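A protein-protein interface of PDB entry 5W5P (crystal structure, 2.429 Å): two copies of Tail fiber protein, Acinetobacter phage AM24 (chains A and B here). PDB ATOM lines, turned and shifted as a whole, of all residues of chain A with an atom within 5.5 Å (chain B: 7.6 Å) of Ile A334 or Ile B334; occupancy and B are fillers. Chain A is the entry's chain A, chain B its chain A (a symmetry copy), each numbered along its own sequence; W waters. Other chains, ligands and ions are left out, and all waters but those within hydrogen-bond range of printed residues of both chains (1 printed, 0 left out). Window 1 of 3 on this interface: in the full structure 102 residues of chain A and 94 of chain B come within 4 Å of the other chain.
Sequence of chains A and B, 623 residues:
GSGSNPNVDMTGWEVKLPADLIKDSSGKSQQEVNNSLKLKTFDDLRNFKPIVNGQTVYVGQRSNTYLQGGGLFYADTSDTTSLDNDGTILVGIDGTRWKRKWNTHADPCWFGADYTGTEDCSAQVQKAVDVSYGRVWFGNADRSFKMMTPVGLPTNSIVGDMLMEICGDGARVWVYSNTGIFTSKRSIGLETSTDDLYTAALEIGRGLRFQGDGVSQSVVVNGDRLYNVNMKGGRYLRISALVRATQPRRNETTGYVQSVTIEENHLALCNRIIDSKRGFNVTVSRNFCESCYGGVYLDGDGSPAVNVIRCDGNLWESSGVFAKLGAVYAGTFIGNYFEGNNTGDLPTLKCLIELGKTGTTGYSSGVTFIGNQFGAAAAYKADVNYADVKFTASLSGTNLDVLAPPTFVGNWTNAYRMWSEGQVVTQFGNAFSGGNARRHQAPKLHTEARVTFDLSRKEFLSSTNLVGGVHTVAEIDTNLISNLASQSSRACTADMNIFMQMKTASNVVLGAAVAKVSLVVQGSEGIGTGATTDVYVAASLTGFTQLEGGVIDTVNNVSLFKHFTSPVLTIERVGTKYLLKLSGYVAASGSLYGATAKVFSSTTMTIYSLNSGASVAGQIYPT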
ATOM      1  N   CYS A 311     -13.065  18.677  -7.462  1.00  0.00           N
ATOM      2  CA  CYS A 311     -13.712  19.958  -7.182  1.00  0.00           C
ATOM      3  C   CYS A 311     -14.289  20.466  -8.498  1.00  0.00           C
ATOM      4  O   CYS A 311     -13.567  21.051  -9.310  1.00  0.00           O
ATOM      5  CB  CYS A 311     -12.729  20.954  -6.573  1.00  0.00           C
ATOM      6  SG  CYS A 311     -11.936  20.397  -5.031  1.00  0.00           S
ATOM      7  N   ASP A 312     -15.588  20.243  -8.708  1.00  0.00           N
ATOM      8  CA  ASP A 312     -16.229  20.503  -9.989  1.00  0.00           C
ATOM      9  C   ASP A 312     -17.393  21.478  -9.839  1.00  0.00           C
ATOM     10  O   ASP A 312     -18.127  21.438  -8.847  1.00  0.00           O
ATOM     11  CB  ASP A 312     -16.729  19.201 -10.624  1.00  0.00           C
ATOM     12  CG  ASP A 312     -15.632  18.156 -10.756  1.00  0.00           C
ATOM     13  OD1 ASP A 312     -14.449  18.542 -10.871  1.00  0.00           O
ATOM     14  OD2 ASP A 312     -15.956  16.946 -10.754  1.00  0.00           O
ATOM     15  N   GLY A 313     -17.550  22.353 -10.831  1.00  0.00           N
ATOM     16  CA  GLY A 313     -18.726  23.198 -10.939  1.00  0.00           C
ATOM     17  C   GLY A 313     -19.034  24.069  -9.741  1.00  0.00           C
ATOM     18  O   GLY A 313     -20.191  24.460  -9.554  1.00  0.00           O
ATOM     19  N   ASN A 314     -18.037  24.390  -8.919  1.00  0.00           N
ATOM     20  CA  ASN A 314     -18.253  25.273  -7.785  1.00  0.00           C
ATOM     21  C   ASN A 314     -18.352  26.727  -8.241  1.00  0.00           C
ATOM     22  O   ASN A 314     -17.861  27.111  -9.306  1.00  0.00           O
ATOM     23  CB  ASN A 314     -17.117  25.149  -6.772  1.00  0.00           C
ATOM     24  CG  ASN A 314     -17.158  23.848  -6.003  1.00  0.00           C
ATOM     25  OD1 ASN A 314     -18.050  23.621  -5.183  1.00  0.00           O
ATOM     26  ND2 ASN A 314     -16.177  22.988  -6.252  1.00  0.00           N
ATOM     27  N   THR A 332      -8.931  16.087  -9.869  1.00  0.00           N
ATOM     28  CA  THR A 332      -9.688  16.637 -10.984  1.00  0.00           C
ATOM     29  C   THR A 332     -10.366  17.929 -10.548  1.00  0.00           C
ATOM     30  O   THR A 332     -10.886  18.020  -9.434  1.00  0.00           O
ATOM     31  CB  THR A 332     -10.732  15.633 -11.509  1.00  0.00           C
ATOM     32  OG1 THR A 332     -11.338  14.942 -10.411  1.00  0.00           O
ATOM     33  CG2 THR A 332     -10.085  14.616 -12.456  1.00  0.00           C
ATOM     34  N   PHE A 333     -10.336  18.933 -11.425  1.00  0.00           N
ATOM     35  CA  PHE A 333     -10.989  20.226 -11.190  1.00  0.00           C
ATOM     36  C   PHE A 333     -11.675  20.628 -12.494  1.00  0.00           C
ATOM     37  O   PHE A 333     -11.029  21.183 -13.389  1.00  0.00           O
ATOM     38  CB  PHE A 333      -9.994  21.293 -10.745  1.00  0.00           C
ATOM     39  CG  PHE A 333      -9.244  20.948  -9.483  1.00  0.00           C
ATOM     40  CD1 PHE A 333      -8.155  20.087  -9.524  1.00  0.00           C
ATOM     41  CD2 PHE A 333      -9.606  21.504  -8.263  1.00  0.00           C
ATOM     42  CE1 PHE A 333      -7.456  19.768  -8.385  1.00  0.00           C
ATOM     43  CE2 PHE A 333      -8.905  21.187  -7.114  1.00  0.00           C
ATOM     44  CZ  PHE A 333      -7.825  20.315  -7.179  1.00  0.00           C
ATOM     45  N   ILE A 334     -12.979  20.368 -12.592  1.00  0.00           N
ATOM     46  CA  ILE A 334     -13.721  20.482 -13.843  1.00  0.00           C
ATOM     47  C   ILE A 334     -14.790  21.556 -13.691  1.00  0.00           C
ATOM     48  O   ILE A 334     -15.717  21.417 -12.883  1.00  0.00           O
ATOM     49  CB  ILE A 334     -14.347  19.144 -14.262  1.00  0.00           C
ATOM     50  CG1 ILE A 334     -13.310  18.016 -14.176  1.00  0.00           C
ATOM     51  CG2 ILE A 334     -14.994  19.260 -15.648  1.00  0.00           C
ATOM     52  CD1 ILE A 334     -13.790  16.690 -14.735  1.00  0.00           C
ATOM     53  N   GLY A 335     -14.667  22.626 -14.472  1.00  0.00           N
ATOM     54  CA  GLY A 335     -15.768  23.551 -14.650  1.00  0.00           C
ATOM     55  C   GLY A 335     -16.045  24.488 -13.500  1.00  0.00           C
ATOM     56  O   GLY A 335     -17.176  24.949 -13.349  1.00  0.00           O
ATOM     57  N   ASN A 336     -15.046  24.787 -12.675  1.00  0.00           N
ATOM     58  CA  ASN A 336     -15.262  25.737 -11.596  1.00  0.00           C
ATOM     59  C   ASN A 336     -15.435  27.151 -12.145  1.00  0.00           C
ATOM     60  O   ASN A 336     -15.016  27.475 -13.261  1.00  0.00           O
ATOM     61  CB  ASN A 336     -14.108  25.696 -10.599  1.00  0.00           C
ATOM     62  CG  ASN A 336     -14.129  24.446  -9.752  1.00  0.00           C
ATOM     63  OD1 ASN A 336     -15.102  24.183  -9.040  1.00  0.00           O
ATOM     64  ND2 ASN A 336     -13.067  23.648  -9.843  1.00  0.00           N
ATOM     65  N   THR A 368      -5.787  16.995 -13.351  1.00  0.00           N
ATOM     66  CA  THR A 368      -6.324  17.509 -14.606  1.00  0.00           C
ATOM     67  C   THR A 368      -7.291  18.651 -14.338  1.00  0.00           C
ATOM     68  O   THR A 368      -8.220  18.507 -13.538  1.00  0.00           O
ATOM     69  CB  THR A 368      -7.030  16.402 -15.397  1.00  0.00           C
ATOM     70  OG1 THR A 368      -6.189  15.244 -15.449  1.00  0.00           O
ATOM     71  CG2 THR A 368      -7.328  16.867 -16.816  1.00  0.00           C
ATOM     72  N   ILE A 370      -9.986  21.019 -16.280  1.00  0.00           N
ATOM     73  CA  ILE A 370     -10.790  21.088 -17.494  1.00  0.00           C
ATOM     74  C   ILE A 370     -11.866  22.150 -17.312  1.00  0.00           C
ATOM     75  O   ILE A 370     -12.652  22.084 -16.361  1.00  0.00           O
ATOM     76  CB  ILE A 370     -11.432  19.732 -17.835  1.00  0.00           C
ATOM     77  CG1 ILE A 370     -10.359  18.641 -17.923  1.00  0.00           C
ATOM     78  CG2 ILE A 370     -12.220  19.828 -19.135  1.00  0.00           C
ATOM     79  CD1 ILE A 370     -10.919  17.255 -18.039  1.00  0.00           C
ATOM     80  N   GLY A 371     -11.890  23.131 -18.213  1.00  0.00           N
ATOM     81  CA  GLY A 371     -13.035  24.016 -18.342  1.00  0.00           C
ATOM     82  C   GLY A 371     -13.301  24.961 -17.190  1.00  0.00           C
ATOM     83  O   GLY A 371     -14.451  25.355 -16.978  1.00  0.00           O
ATOM     84  N   ASN A 372     -12.273  25.346 -16.443  1.00  0.00           N
ATOM     85  CA  ASN A 372     -12.430  26.332 -15.385  1.00  0.00           C
ATOM     86  C   ASN A 372     -12.332  27.742 -15.953  1.00  0.00           C
ATOM     87  O   ASN A 372     -11.656  27.980 -16.957  1.00  0.00           O
ATOM     88  CB  ASN A 372     -11.365  26.139 -14.304  1.00  0.00           C
ATOM     89  CG  ASN A 372     -11.396  24.753 -13.700  1.00  0.00           C
ATOM     90  OD1 ASN A 372     -12.180  24.484 -12.794  1.00  0.00           O
ATOM     91  ND2 ASN A 372     -10.550  23.863 -14.205  1.00  0.00           N
ATOM     92  N   SER B 285     -27.422  19.509 -15.753  1.00  0.00           N
ATOM     93  CA  SER B 285     -26.809  18.188 -15.787  1.00  0.00           C
ATOM     94  C   SER B 285     -27.757  17.117 -15.263  1.00  0.00           C
ATOM     95  O   SER B 285     -28.548  17.354 -14.344  1.00  0.00           O
ATOM     96  CB  SER B 285     -25.518  18.161 -14.962  1.00  0.00           C
ATOM     97  OG  SER B 285     -24.555  19.059 -15.481  1.00  0.00           O
ATOM     98  N   ARG B 286     -27.658  15.924 -15.865  1.00  0.00           N
ATOM     99  CA  ARG B 286     -28.294  14.704 -15.362  1.00  0.00           C
ATOM    100  C   ARG B 286     -29.815  14.858 -15.253  1.00  0.00           C
ATOM    101  O   ARG B 286     -30.433  14.483 -14.257  1.00  0.00           O
ATOM    102  CB  ARG B 286     -27.680  14.283 -14.017  1.00  0.00           C
ATOM    103  CG  ARG B 286     -26.218  13.838 -14.111  1.00  0.00           C
ATOM    104  CD  ARG B 286     -25.507  13.900 -12.759  1.00  0.00           C
ATOM    105  NE  ARG B 286     -25.006  15.239 -12.447  1.00  0.00           N
ATOM    106  CZ  ARG B 286     -23.814  15.705 -12.815  1.00  0.00           C
ATOM    107  NH1 ARG B 286     -22.985  14.943 -13.513  1.00  0.00           N
ATOM    108  NH2 ARG B 286     -23.444  16.936 -12.486  1.00  0.00           N
ATOM    109  N   VAL B 308     -19.079  30.422 -18.078  1.00  0.00           N
ATOM    110  CA  VAL B 308     -19.124  29.052 -17.565  1.00  0.00           C
ATOM    111  C   VAL B 308     -20.515  28.448 -17.715  1.00  0.00           C
ATOM    112  O   VAL B 308     -21.497  28.948 -17.156  1.00  0.00           O
ATOM    113  CB  VAL B 308     -18.665  28.962 -16.096  1.00  0.00           C
ATOM    114  CG1 VAL B 308     -18.625  27.505 -15.639  1.00  0.00           C
ATOM    115  CG2 VAL B 308     -17.313  29.601 -15.932  1.00  0.00           C
ATOM    116  N   ARG B 310     -21.994  24.207 -17.757  1.00  0.00           N
ATOM    117  CA  ARG B 310     -21.730  22.775 -17.769  1.00  0.00           C
ATOM    118  C   ARG B 310     -23.039  22.072 -18.074  1.00  0.00           C
ATOM    119  O   ARG B 310     -24.066  22.380 -17.460  1.00  0.00           O
ATOM    120  CB  ARG B 310     -21.163  22.273 -16.433  1.00  0.00           C
ATOM    121  CG  ARG B 310     -20.101  23.160 -15.812  1.00  0.00           C
ATOM    122  CD  ARG B 310     -20.722  24.285 -14.994  1.00  0.00           C
ATOM    123  NE  ARG B 310     -19.820  24.743 -13.945  1.00  0.00           N
ATOM    124  CZ  ARG B 310     -19.995  25.860 -13.248  1.00  0.00           C
ATOM    125  NH1 ARG B 310     -19.115  26.210 -12.319  1.00  0.00           N
ATOM    126  NH2 ARG B 310     -21.047  26.630 -13.483  1.00  0.00           N
ATOM    127  N   CYS B 311     -23.008  21.147 -19.031  1.00  0.00           N
ATOM    128  CA  CYS B 311     -24.163  20.320 -19.370  1.00  0.00           C
ATOM    129  C   CYS B 311     -23.671  18.880 -19.461  1.00  0.00           C
ATOM    130  O   CYS B 311     -23.125  18.472 -20.493  1.00  0.00           O
ATOM    131  CB  CYS B 311     -24.813  20.780 -20.672  1.00  0.00           C
ATOM    132  SG  CYS B 311     -25.369  22.514 -20.676  1.00  0.00           S
ATOM    133  N   ASP B 312     -23.864  18.111 -18.388  1.00  0.00           N
ATOM    134  CA  ASP B 312     -23.284  16.782 -18.265  1.00  0.00           C
ATOM    135  C   ASP B 312     -24.361  15.725 -18.037  1.00  0.00           C
ATOM    136  O   ASP B 312     -25.349  15.969 -17.338  1.00  0.00           O
ATOM    137  CB  ASP B 312     -22.269  16.733 -17.117  1.00  0.00           C
ATOM    138  CG  ASP B 312     -21.190  17.798 -17.245  1.00  0.00           C
ATOM    139  OD1 ASP B 312     -20.887  18.208 -18.386  1.00  0.00           O
ATOM    140  OD2 ASP B 312     -20.639  18.218 -16.202  1.00  0.00           O
ATOM    141  N   GLY B 313     -24.161  14.553 -18.639  1.00  0.00           N
ATOM    142  CA  GLY B 313     -24.978  13.388 -18.352  1.00  0.00           C
ATOM    143  C   GLY B 313     -26.469  13.554 -18.543  1.00  0.00           C
ATOM    144  O   GLY B 313     -27.248  12.817 -17.928  1.00  0.00           O
ATOM    145  N   ASN B 314     -26.899  14.498 -19.378  1.00  0.00           N
ATOM    146  CA  ASN B 314     -28.316  14.670 -19.653  1.00  0.00           C
ATOM    147  C   ASN B 314     -28.817  13.589 -20.609  1.00  0.00           C
ATOM    148  O   ASN B 314     -28.054  12.988 -21.369  1.00  0.00           O
ATOM    149  CB  ASN B 314     -28.590  16.041 -20.267  1.00  0.00           C
ATOM    150  CG  ASN B 314     -28.459  17.168 -19.268  1.00  0.00           C
ATOM    151  OD1 ASN B 314     -29.272  17.302 -18.351  1.00  0.00           O
ATOM    152  ND2 ASN B 314     -27.438  17.997 -19.449  1.00  0.00           N
ATOM    153  N   GLY B 331     -16.744  26.452 -21.107  1.00  0.00           N
ATOM    154  CA  GLY B 331     -17.874  25.553 -21.273  1.00  0.00           C
ATOM    155  C   GLY B 331     -17.422  24.105 -21.248  1.00  0.00           C
ATOM    156  O   GLY B 331     -16.339  23.772 -21.731  1.00  0.00           O
ATOM    157  N   THR B 332     -18.263  23.246 -20.669  1.00  0.00           N
ATOM    158  CA  THR B 332     -18.010  21.812 -20.630  1.00  0.00           C
ATOM    159  C   THR B 332     -19.300  21.062 -20.932  1.00  0.00           C
ATOM    160  O   THR B 332     -20.373  21.443 -20.461  1.00  0.00           O
ATOM    161  CB  THR B 332     -17.441  21.375 -19.266  1.00  0.00           C
ATOM    162  OG1 THR B 332     -18.101  22.088 -18.214  1.00  0.00           O
ATOM    163  CG2 THR B 332     -15.934  21.640 -19.193  1.00  0.00           C
ATOM    164  N   PHE B 333     -19.191  20.006 -21.741  1.00  0.00           N
ATOM    165  CA  PHE B 333     -20.321  19.140 -22.090  1.00  0.00           C
ATOM    166  C   PHE B 333     -19.819  17.698 -22.030  1.00  0.00           C
ATOM    167  O   PHE B 333     -19.221  17.209 -22.994  1.00  0.00           O
ATOM    168  CB  PHE B 333     -20.883  19.466 -23.470  1.00  0.00           C
ATOM    169  CG  PHE B 333     -21.362  20.887 -23.621  1.00  0.00           C
ATOM    170  CD1 PHE B 333     -20.457  21.914 -23.853  1.00  0.00           C
ATOM    171  CD2 PHE B 333     -22.715  21.195 -23.560  1.00  0.00           C
ATOM    172  CE1 PHE B 333     -20.877  23.215 -24.001  1.00  0.00           C
ATOM    173  CE2 PHE B 333     -23.143  22.501 -23.708  1.00  0.00           C
ATOM    174  CZ  PHE B 333     -22.217  23.514 -23.930  1.00  0.00           C
ATOM    175  N   ILE B 334     -20.076  17.019 -20.913  1.00  0.00           N
ATOM    176  CA  ILE B 334     -19.475  15.724 -20.614  1.00  0.00           C
ATOM    177  C   ILE B 334     -20.575  14.674 -20.523  1.00  0.00           C
ATOM    178  O   ILE B 334     -21.440  14.737 -19.639  1.00  0.00           O
ATOM    179  CB  ILE B 334     -18.648  15.761 -19.320  1.00  0.00           C
ATOM    180  CG1 ILE B 334     -17.709  16.975 -19.320  1.00  0.00           C
ATOM    181  CG2 ILE B 334     -17.911  14.433 -19.110  1.00  0.00           C
ATOM    182  CD1 ILE B 334     -16.730  17.001 -18.160  1.00  0.00           C
ATOM    183  N   GLY B 335     -20.539  13.701 -21.430  1.00  0.00           N
ATOM    184  CA  GLY B 335     -21.320  12.493 -21.261  1.00  0.00           C
ATOM    185  C   GLY B 335     -22.801  12.613 -21.526  1.00  0.00           C
ATOM    186  O   GLY B 335     -23.581  11.832 -20.981  1.00  0.00           O
ATOM    187  N   ASN B 336     -23.219  13.572 -22.346  1.00  0.00           N
ATOM    188  CA  ASN B 336     -24.632  13.674 -22.673  1.00  0.00           C
ATOM    189  C   ASN B 336     -25.068  12.511 -23.562  1.00  0.00           C
ATOM    190  O   ASN B 336     -24.261  11.865 -24.234  1.00  0.00           O
ATOM    191  CB  ASN B 336     -24.935  15.003 -23.359  1.00  0.00           C
ATOM    192  CG  ASN B 336     -24.882  16.167 -22.397  1.00  0.00           C
ATOM    193  OD1 ASN B 336     -25.624  16.204 -21.411  1.00  0.00           O
ATOM    194  ND2 ASN B 336     -23.984  17.114 -22.659  1.00  0.00           N
ATOM    195  N   TYR B 337     -26.372  12.249 -23.544  1.00  0.00           N
ATOM    196  CA  TYR B 337     -26.993  11.179 -24.316  1.00  0.00           C
ATOM    197  C   TYR B 337     -28.007  11.825 -25.253  1.00  0.00           C
ATOM    198  O   TYR B 337     -29.075  12.269 -24.812  1.00  0.00           O
ATOM    199  CB  TYR B 337     -27.646  10.158 -23.380  1.00  0.00           C
ATOM    200  CG  TYR B 337     -28.369   8.995 -24.041  1.00  0.00           C
ATOM    201  CD1 TYR B 337     -29.633   9.161 -24.596  1.00  0.00           C
ATOM    202  CD2 TYR B 337     -27.810   7.722 -24.060  1.00  0.00           C
ATOM    203  CE1 TYR B 337     -30.301   8.108 -25.180  1.00  0.00           C
ATOM    204  CE2 TYR B 337     -28.476   6.656 -24.640  1.00  0.00           C
ATOM    205  CZ  TYR B 337     -29.723   6.855 -25.198  1.00  0.00           C
ATOM    206  OH  TYR B 337     -30.397   5.803 -25.777  1.00  0.00           O
ATOM    207  N   THR B 368     -15.016  22.330 -24.053  1.00  0.00           N
ATOM    208  CA  THR B 368     -14.558  20.949 -24.170  1.00  0.00           C
ATOM    209  C   THR B 368     -15.745  19.999 -24.185  1.00  0.00           C
ATOM    210  O   THR B 368     -16.603  20.059 -23.298  1.00  0.00           O
ATOM    211  CB  THR B 368     -13.611  20.585 -23.023  1.00  0.00           C
ATOM    212  OG1 THR B 368     -12.622  21.611 -22.876  1.00  0.00           O
ATOM    213  CG2 THR B 368     -12.915  19.260 -23.305  1.00  0.00           C
ATOM    214  N   PHE B 369     -15.779  19.115 -25.183  1.00  0.00           N
ATOM    215  CA  PHE B 369     -16.795  18.073 -25.316  1.00  0.00           C
ATOM    216  C   PHE B 369     -16.143  16.720 -25.079  1.00  0.00           C
ATOM    217  O   PHE B 369     -15.256  16.320 -25.836  1.00  0.00           O
ATOM    218  CB  PHE B 369     -17.439  18.106 -26.701  1.00  0.00           C
ATOM    219  CG  PHE B 369     -18.185  19.368 -26.990  1.00  0.00           C
ATOM    220  CD1 PHE B 369     -17.518  20.491 -27.452  1.00  0.00           C
ATOM    221  CD2 PHE B 369     -19.558  19.433 -26.799  1.00  0.00           C
ATOM    222  CE1 PHE B 369     -18.204  21.659 -27.720  1.00  0.00           C
ATOM    223  CE2 PHE B 369     -20.254  20.599 -27.069  1.00  0.00           C
ATOM    224  CZ  PHE B 369     -19.577  21.713 -27.531  1.00  0.00           C
ATOM    225  N   ILE B 370     -16.588  16.011 -24.043  1.00  0.00           N
ATOM    226  CA  ILE B 370     -16.012  14.727 -23.662  1.00  0.00           C
ATOM    227  C   ILE B 370     -17.129  13.698 -23.554  1.00  0.00           C
ATOM    228  O   ILE B 370     -18.090  13.899 -22.804  1.00  0.00           O
ATOM    229  CB  ILE B 370     -15.239  14.815 -22.335  1.00  0.00           C
ATOM    230  CG1 ILE B 370     -14.177  15.918 -22.409  1.00  0.00           C
ATOM    231  CG2 ILE B 370     -14.608  13.471 -21.997  1.00  0.00           C
ATOM    232  CD1 ILE B 370     -13.524  16.215 -21.092  1.00  0.00           C
ATOM    233  N   GLY B 371     -17.008  12.609 -24.311  1.00  0.00           N
ATOM    234  CA  GLY B 371     -17.820  11.426 -24.077  1.00  0.00           C
ATOM    235  C   GLY B 371     -19.302  11.550 -24.354  1.00  0.00           C
ATOM    236  O   GLY B 371     -20.099  10.832 -23.743  1.00  0.00           O
ATOM    237  N   ASN B 372     -19.700  12.432 -25.264  1.00  0.00           N
ATOM    238  CA  ASN B 372     -21.095  12.537 -25.662  1.00  0.00           C
ATOM    239  C   ASN B 372     -21.417  11.518 -26.748  1.00  0.00           C
ATOM    240  O   ASN B 372     -20.551  11.134 -27.538  1.00  0.00           O
ATOM    241  CB  ASN B 372     -21.408  13.946 -26.169  1.00  0.00           C
ATOM    242  CG  ASN B 372     -21.103  15.012 -25.142  1.00  0.00           C
ATOM    243  OD1 ASN B 372     -21.918  15.287 -24.265  1.00  0.00           O
ATOM    244  ND2 ASN B 372     -19.923  15.615 -25.240  1.00  0.00           N
ATOM    245  N   GLN B 373     -22.669  11.073 -26.777  1.00  0.00           N
ATOM    246  CA  GLN B 373     -23.187  10.295 -27.895  1.00  0.00           C
ATOM    247  C   GLN B 373     -24.162  11.160 -28.673  1.00  0.00           C
ATOM    248  O   GLN B 373     -25.201  11.564 -28.141  1.00  0.00           O
ATOM    249  CB  GLN B 373     -23.879   9.011 -27.444  1.00  0.00           C
ATOM    250  CG  GLN B 373     -24.616   8.314 -28.578  1.00  0.00           C
ATOM    251  CD  GLN B 373     -25.513   7.188 -28.098  1.00  0.00           C
ATOM    252  OE1 GLN B 373     -26.716   7.377 -27.904  1.00  0.00           O
ATOM    253  NE2 GLN B 373     -24.938   6.005 -27.927  1.00  0.00           N
ATOM    254  N   ASN B 411     -15.910  11.430 -28.039  1.00  0.00           N
ATOM    255  CA  ASN B 411     -17.325  11.490 -28.378  1.00  0.00           C
ATOM    256  C   ASN B 411     -17.665  10.470 -29.462  1.00  0.00           C
ATOM    257  O   ASN B 411     -16.788   9.920 -30.127  1.00  0.00           O
ATOM    258  CB  ASN B 411     -17.715  12.892 -28.852  1.00  0.00           C
ATOM    259  CG  ASN B 411     -17.346  13.970 -27.849  1.00  0.00           C
ATOM    260  OD1 ASN B 411     -18.081  14.219 -26.888  1.00  0.00           O
ATOM    261  ND2 ASN B 411     -16.195  14.616 -28.065  1.00  0.00           N
HETATM  262  O   HOH W   1     -16.848  24.614 -17.728  1.00  0.00           O
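Of chain B, only Ile B334 comes within 4 Å of Ile A334. Of the printed residues of chain B, Gly A335 touches Val B308 and Arg B310. Of the printed residues of chain A, Val B308 touches Gly A335. Of chain A, only Ile A334 (3.8 Å) comes within 4 Å of Ile B334. Phe B369 touches none of the printed residues of chain A. Asn B372 touches none of the printed residues of chain A. The nearest residue of chain A that does not touch Ile B334 is Ile A370 (5.4 Å).
The backbone carbonyl oxygen (O) of Cys B311 sits at hydrogen-bond distance from the backbone NH (N) of Ile B334. OD1 of Asn A336 sits at hydrogen-bond distance from N of Asn A314, at 2.9 Å. The side-chain amide nitrogen (ND2) of Asn A336 is in hydrogen-bond range of the backbone carbonyl oxygen (O) of Cys A311, at 2.7 Å. The backbone carbonyl oxygen (O) of Cys A311 sits at hydrogen-bond distance from the backbone NH (N) of Ile A334 (3.4 Å). N of Ile A334 lies within hydrogen-bond range of OD1 of Asp A312. O of Ile A334 is in hydrogen-bond range of N of Gly A313.
Of the 13 printed residues of chain A, 6 touch a printed residue of chain B. Hydrophobic or aromatic side chains of chain A within 4 Å of the printed part of chain B: Ile A334. Along chain A the printed residues that touch a printed residue of chain B span positions 313 to 371. Of the 22 printed residues of chain B, 4 touch a printed residue of chain A. Printed residues of chain B that touch a printed residue of chain A: Val B308, Arg B310, Thr B332 and Ile B334. Hydrophobic or aromatic side chains of chain B within 4 Å of the printed part of chain A: Val B308 and Ile B334. Among the printed residues, no Asp or Glu carboxylate lies within 4 Å of a Lys or Arg side-chain nitrogen of the other chain.
Water W1 lies within hydrogen-bond range of the backbone carbonyl oxygen (O) of Gly A371 (2.6 Å) and the side-chain hydroxyl (OG1) of Thr B332 (2.9 Å).
Ile A334 touches its own counterpart, Ile B334. Gly A371 touches Thr B332, but with the chains exchanged Thr A332 does not touch Gly B371 (13.9 Å). Positions printed for both chains: 311, 312, 313, 314, 332, 333, 334, 335, 336, 368, 370, 371 and 372. Of the 7 pairs that touch across the chains among the printed residues, 1 has its exchanged pair printed and touching as well.
Among the printed residues, merely in contact across the chains: Ile A334 with Ile B334, Gly A335 with Val B308, Asn A336 with Arg B310 and Gly A371 with Thr B332.
The backbone carbonyl oxygen (O) of Gly A335 is in hydrogen-bond range of the guanidinium group (NH1) of Arg B310, 2.5 Å away. O of Asn A314 sits at hydrogen-bond distance from NH1 of Arg B310. NH1 of Arg B310 sits close to O of Gly A313, at 3.4 Å.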
